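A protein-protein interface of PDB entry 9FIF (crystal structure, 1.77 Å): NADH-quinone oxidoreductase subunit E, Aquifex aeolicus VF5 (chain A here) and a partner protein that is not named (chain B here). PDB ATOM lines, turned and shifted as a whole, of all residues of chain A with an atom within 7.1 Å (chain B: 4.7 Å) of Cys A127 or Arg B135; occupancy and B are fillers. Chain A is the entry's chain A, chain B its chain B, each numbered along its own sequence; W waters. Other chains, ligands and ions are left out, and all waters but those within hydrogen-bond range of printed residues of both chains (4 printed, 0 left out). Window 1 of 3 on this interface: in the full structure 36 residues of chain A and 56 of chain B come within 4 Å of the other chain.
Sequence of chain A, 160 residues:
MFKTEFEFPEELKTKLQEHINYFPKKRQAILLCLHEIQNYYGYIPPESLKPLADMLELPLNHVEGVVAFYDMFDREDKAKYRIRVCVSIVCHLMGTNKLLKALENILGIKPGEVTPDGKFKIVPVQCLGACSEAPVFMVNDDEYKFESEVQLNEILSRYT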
ATOM      1  N   HIS A  35      34.057 -13.738 -16.598  1.00  0.00           N
ATOM      2  CA  HIS A  35      33.782 -12.587 -15.750  1.00  0.00           C
ATOM      3  C   HIS A  35      35.075 -11.820 -15.458  1.00  0.00           C
ATOM      4  O   HIS A  35      35.100 -10.593 -15.514  1.00  0.00           O
ATOM      5  CB  HIS A  35      33.105 -13.026 -14.445  1.00  0.00           C
ATOM      6  CG  HIS A  35      31.642 -13.303 -14.549  1.00  0.00           C
ATOM      7  ND1 HIS A  35      30.728 -12.336 -14.910  1.00  0.00           N
ATOM      8  CD2 HIS A  35      30.921 -14.403 -14.252  1.00  0.00           C
ATOM      9  CE1 HIS A  35      29.504 -12.862 -14.877  1.00  0.00           C
ATOM     10  NE2 HIS A  35      29.596 -14.113 -14.451  1.00  0.00           N
ATOM     11  N   MET A  72      25.491 -11.592 -20.025  1.00  0.00           N
ATOM     12  CA  MET A  72      26.308 -10.620 -19.314  1.00  0.00           C
ATOM     13  C   MET A  72      27.574 -10.265 -20.098  1.00  0.00           C
ATOM     14  O   MET A  72      28.084  -9.165 -19.926  1.00  0.00           O
ATOM     15  CB  MET A  72      26.690 -11.107 -17.912  1.00  0.00           C
ATOM     16  CG  MET A  72      25.537 -11.034 -16.941  1.00  0.00           C
ATOM     17  SD  MET A  72      25.978 -11.434 -15.238  1.00  0.00           S
ATOM     18  CE  MET A  72      26.927  -9.976 -14.776  1.00  0.00           C
ATOM     19  N   CYS A  86      17.262  -2.291 -15.336  1.00  0.00           N
ATOM     20  CA  CYS A  86      16.221  -3.299 -15.430  1.00  0.00           C
ATOM     21  C   CYS A  86      15.058  -2.769 -16.258  1.00  0.00           C
ATOM     22  O   CYS A  86      14.577  -1.668 -16.001  1.00  0.00           O
ATOM     23  CB  CYS A  86      15.749  -3.711 -14.054  1.00  0.00           C
ATOM     24  SG  CYS A  86      14.419  -4.927 -14.139  1.00  0.00           S
ATOM     25  N   VAL A  87      14.626  -3.555 -17.255  1.00  0.00           N
ATOM     26  CA  VAL A  87      13.511  -3.176 -18.114  1.00  0.00           C
ATOM     27  C   VAL A  87      12.347  -4.161 -17.969  1.00  0.00           C
ATOM     28  O   VAL A  87      11.423  -4.124 -18.775  1.00  0.00           O
ATOM     29  CB  VAL A  87      13.943  -3.053 -19.592  1.00  0.00           C
ATOM     30  CG1 VAL A  87      14.982  -1.953 -19.774  1.00  0.00           C
ATOM     31  CG2 VAL A  87      14.443  -4.374 -20.183  1.00  0.00           C
ATOM     32  N   SER A  88      12.367  -5.027 -16.949  1.00  0.00           N
ATOM     33  CA  SER A  88      11.304  -6.006 -16.754  1.00  0.00           C
ATOM     34  C   SER A  88      10.102  -5.370 -16.052  1.00  0.00           C
ATOM     35  O   SER A  88      10.113  -4.188 -15.728  1.00  0.00           O
ATOM     36  CB  SER A  88      11.792  -7.211 -15.990  1.00  0.00           C
ATOM     37  OG  SER A  88      12.732  -7.945 -16.750  1.00  0.00           O
ATOM     38  N   ILE A  89       9.065  -6.181 -15.829  1.00  0.00           N
ATOM     39  CA  ILE A  89       7.723  -5.720 -15.492  1.00  0.00           C
ATOM     40  C   ILE A  89       7.718  -4.747 -14.309  1.00  0.00           C
ATOM     41  O   ILE A  89       7.100  -3.685 -14.418  1.00  0.00           O
ATOM     42  CB  ILE A  89       6.786  -6.915 -15.242  1.00  0.00           C
ATOM     43  CG1 ILE A  89       5.375  -6.472 -14.804  1.00  0.00           C
ATOM     44  CG2 ILE A  89       7.357  -7.901 -14.234  1.00  0.00           C
ATOM     45  CD1 ILE A  89       4.563  -5.880 -15.920  1.00  0.00           C
ATOM     46  N   VAL A  90       8.348  -5.094 -13.177  1.00  0.00           N
ATOM     47  CA  VAL A  90       8.138  -4.294 -11.972  1.00  0.00           C
ATOM     48  C   VAL A  90       8.834  -2.942 -12.132  1.00  0.00           C
ATOM     49  O   VAL A  90       8.221  -1.896 -11.896  1.00  0.00           O
ATOM     50  CB  VAL A  90       8.514  -4.997 -10.655  1.00  0.00           C
ATOM     51  CG1 VAL A  90       8.037  -4.201  -9.445  1.00  0.00           C
ATOM     52  CG2 VAL A  90       7.938  -6.402 -10.603  1.00  0.00           C
ATOM     53  N   CYS A  91      10.076  -2.941 -12.628  1.00  0.00           N
ATOM     54  CA  CYS A  91      10.768  -1.677 -12.830  1.00  0.00           C
ATOM     55  C   CYS A  91      10.034  -0.806 -13.846  1.00  0.00           C
ATOM     56  O   CYS A  91       9.986   0.421 -13.683  1.00  0.00           O
ATOM     57  CB  CYS A  91      12.246  -1.900 -13.125  1.00  0.00           C
ATOM     58  SG  CYS A  91      13.095  -2.610 -11.691  1.00  0.00           S
ATOM     59  N   VAL A 125      18.643  -4.798 -19.035  1.00  0.00           N
ATOM     60  CA  VAL A 125      18.700  -6.142 -18.488  1.00  0.00           C
ATOM     61  C   VAL A 125      17.314  -6.550 -17.999  1.00  0.00           C
ATOM     62  O   VAL A 125      16.440  -5.714 -17.764  1.00  0.00           O
ATOM     63  CB  VAL A 125      19.746  -6.325 -17.367  1.00  0.00           C
ATOM     64  CG1 VAL A 125      21.153  -6.076 -17.878  1.00  0.00           C
ATOM     65  CG2 VAL A 125      19.440  -5.467 -16.136  1.00  0.00           C
ATOM     66  N   GLN A 126      17.132  -7.871 -17.898  1.00  0.00           N
ATOM     67  CA  GLN A 126      15.962  -8.463 -17.285  1.00  0.00           C
ATOM     68  C   GLN A 126      16.046  -8.307 -15.763  1.00  0.00           C
ATOM     69  O   GLN A 126      17.083  -7.939 -15.225  1.00  0.00           O
ATOM     70  CB  GLN A 126      15.891  -9.926 -17.718  1.00  0.00           C
ATOM     71  CG  GLN A 126      15.814 -10.120 -19.234  1.00  0.00           C
ATOM     72  CD  GLN A 126      14.662  -9.371 -19.868  1.00  0.00           C
ATOM     73  OE1 GLN A 126      13.485  -9.636 -19.592  1.00  0.00           O
ATOM     74  NE2 GLN A 126      14.991  -8.426 -20.742  1.00  0.00           N
ATOM     75  N   CYS A 127      14.946  -8.640 -15.080  1.00  0.00           N
ATOM     76  CA  CYS A 127      14.796  -8.496 -13.640  1.00  0.00           C
ATOM     77  C   CYS A 127      16.093  -8.813 -12.896  1.00  0.00           C
ATOM     78  O   CYS A 127      16.676  -9.907 -13.041  1.00  0.00           O
ATOM     79  CB  CYS A 127      13.696  -9.414 -13.134  1.00  0.00           C
ATOM     80  SG  CYS A 127      13.413  -9.295 -11.346  1.00  0.00           S
ATOM     81  N   LEU A 128      16.528  -7.836 -12.086  1.00  0.00           N
ATOM     82  CA  LEU A 128      17.748  -7.931 -11.304  1.00  0.00           C
ATOM     83  C   LEU A 128      17.496  -8.499  -9.908  1.00  0.00           C
ATOM     84  O   LEU A 128      18.389  -8.497  -9.070  1.00  0.00           O
ATOM     85  CB  LEU A 128      18.369  -6.534 -11.219  1.00  0.00           C
ATOM     86  CG  LEU A 128      19.041  -6.023 -12.495  1.00  0.00           C
ATOM     87  CD1 LEU A 128      19.365  -4.532 -12.411  1.00  0.00           C
ATOM     88  CD2 LEU A 128      20.286  -6.835 -12.778  1.00  0.00           C
ATOM     89  N   GLY A 129      16.272  -8.922  -9.615  1.00  0.00           N
ATOM     90  CA  GLY A 129      15.984  -9.472  -8.299  1.00  0.00           C
ATOM     91  C   GLY A 129      16.098  -8.434  -7.181  1.00  0.00           C
ATOM     92  O   GLY A 129      16.607  -8.751  -6.113  1.00  0.00           O
ATOM     93  N   ALA A 130      15.581  -7.218  -7.421  1.00  0.00           N
ATOM     94  CA  ALA A 130      15.489  -6.193  -6.387  1.00  0.00           C
ATOM     95  C   ALA A 130      14.209  -5.370  -6.553  1.00  0.00           C
ATOM     96  O   ALA A 130      14.212  -4.169  -6.299  1.00  0.00           O
ATOM     97  CB  ALA A 130      16.726  -5.312  -6.412  1.00  0.00           C
ATOM     98  N   CYS A 131      13.120  -6.063  -6.917  1.00  0.00           N
ATOM     99  CA  CYS A 131      11.923  -5.463  -7.486  1.00  0.00           C
ATOM    100  C   CYS A 131      11.225  -4.534  -6.487  1.00  0.00           C
ATOM    101  O   CYS A 131      10.565  -3.572  -6.880  1.00  0.00           O
ATOM    102  CB  CYS A 131      10.965  -6.544  -7.997  1.00  0.00           C
ATOM    103  SG  CYS A 131      11.779  -7.934  -8.840  1.00  0.00           S
ATOM    104  N   ALA B  93      20.807 -20.858  -6.333  1.00  0.00           N
ATOM    105  CA  ALA B  93      20.715 -19.437  -6.032  1.00  0.00           C
ATOM    106  C   ALA B  93      20.636 -18.603  -7.315  1.00  0.00           C
ATOM    107  O   ALA B  93      21.166 -17.494  -7.400  1.00  0.00           O
ATOM    108  CB  ALA B  93      21.905 -19.050  -5.176  1.00  0.00           C
ATOM    109  N   ASP B  94      19.939 -19.127  -8.334  1.00  0.00           N
ATOM    110  CA  ASP B  94      19.874 -18.433  -9.606  1.00  0.00           C
ATOM    111  C   ASP B  94      18.811 -17.333  -9.633  1.00  0.00           C
ATOM    112  O   ASP B  94      18.880 -16.503 -10.522  1.00  0.00           O
ATOM    113  CB  ASP B  94      19.662 -19.350 -10.797  1.00  0.00           C
ATOM    114  CG  ASP B  94      20.083 -18.699 -12.107  1.00  0.00           C
ATOM    115  OD1 ASP B  94      21.292 -18.426 -12.227  1.00  0.00           O
ATOM    116  OD2 ASP B  94      19.183 -18.399 -12.952  1.00  0.00           O
ATOM    117  N   GLU B  95      17.826 -17.390  -8.722  1.00  0.00           N
ATOM    118  CA  GLU B  95      16.718 -16.440  -8.559  1.00  0.00           C
ATOM    119  C   GLU B  95      16.693 -15.312  -9.595  1.00  0.00           C
ATOM    120  O   GLU B  95      17.275 -14.246  -9.377  1.00  0.00           O
ATOM    121  CB  GLU B  95      16.786 -15.874  -7.138  1.00  0.00           C
ATOM    122  CG  GLU B  95      15.714 -14.828  -6.837  1.00  0.00           C
ATOM    123  CD  GLU B  95      15.610 -14.511  -5.358  1.00  0.00           C
ATOM    124  OE1 GLU B  95      16.489 -13.775  -4.847  1.00  0.00           O
ATOM    125  OE2 GLU B  95      14.652 -15.015  -4.716  1.00  0.00           O
ATOM    126  N   SER B  96      15.989 -15.540 -10.720  1.00  0.00           N
ATOM    127  CA  SER B  96      15.926 -14.569 -11.806  1.00  0.00           C
ATOM    128  C   SER B  96      14.504 -14.337 -12.325  1.00  0.00           C
ATOM    129  O   SER B  96      14.311 -13.616 -13.302  1.00  0.00           O
ATOM    130  CB  SER B  96      16.837 -14.982 -12.922  1.00  0.00           C
ATOM    131  OG  SER B  96      18.172 -14.781 -12.504  1.00  0.00           O
ATOM    132  N   GLU B  97      13.508 -14.919 -11.667  1.00  0.00           N
ATOM    133  CA  GLU B  97      12.142 -14.721 -12.107  1.00  0.00           C
ATOM    134  C   GLU B  97      11.692 -13.308 -11.756  1.00  0.00           C
ATOM    135  O   GLU B  97      11.928 -12.860 -10.630  1.00  0.00           O
ATOM    136  CB  GLU B  97      11.180 -15.712 -11.467  1.00  0.00           C
ATOM    137  CG  GLU B  97       9.845 -15.671 -12.204  1.00  0.00           C
ATOM    138  CD  GLU B  97       8.828 -16.715 -11.847  1.00  0.00           C
ATOM    139  OE1 GLU B  97       9.150 -17.655 -11.080  1.00  0.00           O
ATOM    140  OE2 GLU B  97       7.699 -16.542 -12.357  1.00  0.00           O
ATOM    141  N   PRO B  98      11.002 -12.569 -12.660  1.00  0.00           N
ATOM    142  CA  PRO B  98      10.468 -11.257 -12.306  1.00  0.00           C
ATOM    143  C   PRO B  98       9.665 -11.258 -11.016  1.00  0.00           C
ATOM    144  O   PRO B  98       8.807 -12.126 -10.795  1.00  0.00           O
ATOM    145  CB  PRO B  98       9.638 -10.861 -13.539  1.00  0.00           C
ATOM    146  CG  PRO B  98      10.406 -11.502 -14.670  1.00  0.00           C
ATOM    147  CD  PRO B  98      10.782 -12.873 -14.084  1.00  0.00           C
ATOM    148  N   GLY B  99       9.972 -10.263 -10.175  1.00  0.00           N
ATOM    149  CA  GLY B  99       9.305 -10.074  -8.902  1.00  0.00           C
ATOM    150  C   GLY B  99      10.011 -10.780  -7.747  1.00  0.00           C
ATOM    151  O   GLY B  99       9.673 -10.537  -6.589  1.00  0.00           O
ATOM    152  N   TYR B 133      25.132 -22.332  -6.928  1.00  0.00           N
ATOM    153  CA  TYR B 133      25.100 -21.657  -8.209  1.00  0.00           C
ATOM    154  C   TYR B 133      24.324 -20.357  -8.024  1.00  0.00           C
ATOM    155  O   TYR B 133      23.107 -20.381  -7.829  1.00  0.00           O
ATOM    156  CB  TYR B 133      24.478 -22.549  -9.282  1.00  0.00           C
ATOM    157  CG  TYR B 133      24.598 -22.026 -10.705  1.00  0.00           C
ATOM    158  CD1 TYR B 133      23.697 -21.090 -11.208  1.00  0.00           C
ATOM    159  CD2 TYR B 133      25.634 -22.448 -11.537  1.00  0.00           C
ATOM    160  CE1 TYR B 133      23.818 -20.610 -12.506  1.00  0.00           C
ATOM    161  CE2 TYR B 133      25.744 -21.991 -12.845  1.00  0.00           C
ATOM    162  CZ  TYR B 133      24.833 -21.065 -13.325  1.00  0.00           C
ATOM    163  OH  TYR B 133      24.935 -20.613 -14.605  1.00  0.00           O
ATOM    164  N   ILE B 134      25.045 -19.236  -8.055  1.00  0.00           N
ATOM    165  CA  ILE B 134      24.436 -17.932  -7.838  1.00  0.00           C
ATOM    166  C   ILE B 134      24.478 -17.134  -9.132  1.00  0.00           C
ATOM    167  O   ILE B 134      25.500 -17.064  -9.821  1.00  0.00           O
ATOM    168  CB  ILE B 134      25.086 -17.192  -6.650  1.00  0.00           C
ATOM    169  CG1 ILE B 134      24.324 -15.889  -6.311  1.00  0.00           C
ATOM    170  CG2 ILE B 134      26.584 -16.928  -6.854  1.00  0.00           C
ATOM    171  CD1 ILE B 134      24.689 -15.325  -4.952  1.00  0.00           C
ATOM    172  N   ARG B 135      23.354 -16.465  -9.431  1.00  0.00           N
ATOM    173  CA  ARG B 135      23.264 -15.704 -10.660  1.00  0.00           C
ATOM    174  C   ARG B 135      24.378 -14.663 -10.672  1.00  0.00           C
ATOM    175  O   ARG B 135      24.806 -14.160  -9.630  1.00  0.00           O
ATOM    176  CB  ARG B 135      21.895 -15.035 -10.821  1.00  0.00           C
ATOM    177  CG  ARG B 135      21.666 -13.937  -9.799  1.00  0.00           C
ATOM    178  CD  ARG B 135      20.307 -13.310  -9.940  1.00  0.00           C
ATOM    179  NE  ARG B 135      20.177 -12.578 -11.199  1.00  0.00           N
ATOM    180  CZ  ARG B 135      19.114 -11.863 -11.565  1.00  0.00           C
ATOM    181  NH1 ARG B 135      18.013 -11.876 -10.819  1.00  0.00           N
ATOM    182  NH2 ARG B 135      19.157 -11.181 -12.699  1.00  0.00           N
ATOM    183  N   GLY B 136      24.842 -14.343 -11.879  1.00  0.00           N
ATOM    184  CA  GLY B 136      25.949 -13.425 -12.062  1.00  0.00           C
ATOM    185  C   GLY B 136      25.594 -12.002 -11.633  1.00  0.00           C
ATOM    186  O   GLY B 136      26.501 -11.255 -11.290  1.00  0.00           O
ATOM    187  N   GLU B 137      24.296 -11.637 -11.655  1.00  0.00           N
ATOM    188  CA  GLU B 137      23.860 -10.287 -11.293  1.00  0.00           C
ATOM    189  C   GLU B 137      23.736 -10.109  -9.768  1.00  0.00           C
ATOM    190  O   GLU B 137      23.299  -9.048  -9.306  1.00  0.00           O
ATOM    191  CB  GLU B 137      22.561  -9.860 -11.984  1.00  0.00           C
ATOM    192  CG  GLU B 137      22.556 -10.005 -13.505  1.00  0.00           C
ATOM    193  CD  GLU B 137      22.300 -11.419 -14.045  1.00  0.00           C
ATOM    194  OE1 GLU B 137      22.125 -12.405 -13.271  1.00  0.00           O
ATOM    195  OE2 GLU B 137      22.249 -11.524 -15.285  1.00  0.00           O
ATOM    196  N   TYR B 138      24.173 -11.117  -8.989  1.00  0.00           N
ATOM    197  CA  TYR B 138      24.302 -11.033  -7.538  1.00  0.00           C
ATOM    198  C   TYR B 138      25.771 -11.074  -7.127  1.00  0.00           C
ATOM    199  O   TYR B 138      26.213 -11.993  -6.425  1.00  0.00           O
ATOM    200  CB  TYR B 138      23.568 -12.189  -6.849  1.00  0.00           C
ATOM    201  CG  TYR B 138      22.051 -12.144  -6.780  1.00  0.00           C
ATOM    202  CD1 TYR B 138      21.333 -11.005  -7.153  1.00  0.00           C
ATOM    203  CD2 TYR B 138      21.332 -13.249  -6.338  1.00  0.00           C
ATOM    204  CE1 TYR B 138      19.953 -10.972  -7.068  1.00  0.00           C
ATOM    205  CE2 TYR B 138      19.949 -13.221  -6.239  1.00  0.00           C
ATOM    206  CZ  TYR B 138      19.260 -12.076  -6.610  1.00  0.00           C
ATOM    207  OH  TYR B 138      17.901 -12.029  -6.512  1.00  0.00           O
ATOM    208  N   GLY B 176      26.542 -17.652 -12.352  1.00  0.00           N
ATOM    209  CA  GLY B 176      25.854 -17.562 -13.622  1.00  0.00           C
ATOM    210  C   GLY B 176      26.380 -16.378 -14.418  1.00  0.00           C
ATOM    211  O   GLY B 176      27.279 -15.672 -13.953  1.00  0.00           O
HETATM  212  O   HOH W   1      14.913 -11.940 -10.020  1.00  0.00           O
HETATM  213  O   HOH W   2      19.495  -9.406 -15.333  1.00  0.00           O
HETATM  214  O   HOH W   3      20.885  -7.840  -8.726  1.00  0.00           O
HETATM  215  O   HOH W   4      15.858 -11.978 -14.699  1.00  0.00           O
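A ring nitrogen (NE2) of His A35 is in hydrogen-bond range of the backbone carbonyl oxygen (O) of Gly B176, at 2.8 Å.
The side-chain sulfur (SG) of Cys A127 lies close to the backbone NH (N) of Gly B99.
NH2 of Arg B135 lies within hydrogen-bond range of O of Cys A127.
SG of Cys A131 sits close to N of Gly B99, 3.2 Å away.
The side-chain sulfur (SD) of Met A72 lies close to the side-chain carboxylate (OE2) of Glu B137 (3.7 Å).
SG of Cys A127 sits close to N of Gly A129 (3.4 Å).
The backbone NH of Arg B135 lies within hydrogen-bond range of the backbone carbonyl oxygen of Ala B93 (3.2 Å).
The side-chain hydroxyl (OG) of Ser B96 sits close to the guanidinium group (NE) of Arg B135, at 3.3 Å.
N of Gly B176 lies within hydrogen-bond range of O of Ile B134 (2.8 Å).
NE of Arg B135 lies within salt-bridge range of OE1 of Glu B137.
The backbone carbonyl oxygen of Gly B176 lies close to the backbone NH of Gly B136 (3.5 Å).
Met A72 touches Gly B136 (SD to C, 3.7 Å).
Ile A89 touches Pro B98.
O of Glu B97 touches SG of Cys A127, at 3.9 Å.
Pro B98 touches Cys A127.
Leu A128 touches Arg B135 (C to NH1, 3.5 Å).
Leu A128 touches Glu B137.
CE1 of Tyr B138 touches O of Leu A128, at 3.5 Å.
Arg B135 touches Gly A129 (NH1 to N, 3.6 Å).
Gly A129 touches Tyr B138 (O to OH, 3.5 Å).
Cys A127 touches just these residues of chain B: Glu B97, Pro B98, Gly B99 and Arg B135.
Arg B135 touches three residues of chain A.
Printed residues of chain A within 4 Å of Gly B99: Cys A127 (3.8 Å) and Cys A131 (3.2 Å).
Of the printed residues of chain B, Leu A128 touches Arg B135 (3.5 Å), Glu B137 (3.9 Å) and Tyr B138 (3.5 Å).
Of the printed residues of chain A, Pro B98 touches Ile A89 and Cys A127.
Val A87 touches none of the printed residues of chain B.
Cys A86 touches none of the printed residues of chain B.
Printed residues of chain B that touch a printed residue of chain A: Glu B97, Pro B98, Gly B99, Arg B135, Gly B136, Glu B137, Tyr B138 and Gly B176.
Hydrophobic or aromatic side chains of chain B that line the printed part of chain A: Pro B98 and Tyr B138.
Of the 15 printed residues of chain A, 7 touch a printed residue of chain B.
Printed residues of chain A that touch a printed residue of chain B: His A35, Met A72, Ile A89, Cys A127, Leu A128, Gly A129 and Cys A131.
Among the printed residues, 14 pairs touch across the chains.
Water W3 bridges the backbone carbonyl oxygen (O) of Leu A128 and the backbone carbonyl oxygen (O) of Glu B137.
Water W4 lies within hydrogen-bond range of the backbone carbonyl oxygen (O) of Ser B96 (2.7 Å) and the backbone carbonyl oxygen (O) of Cys A127 (2.8 Å).
Water W2 lies within hydrogen-bond range of O of Gln A126 (2.8 Å), NH2 of Arg B135 (3.2 Å) and OE2 of Glu B137 (3.5 Å).
Water W1 lies within hydrogen-bond range of O of Glu B97, NH1 of Arg B135, N of Gly A129 and O of Glu B95.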
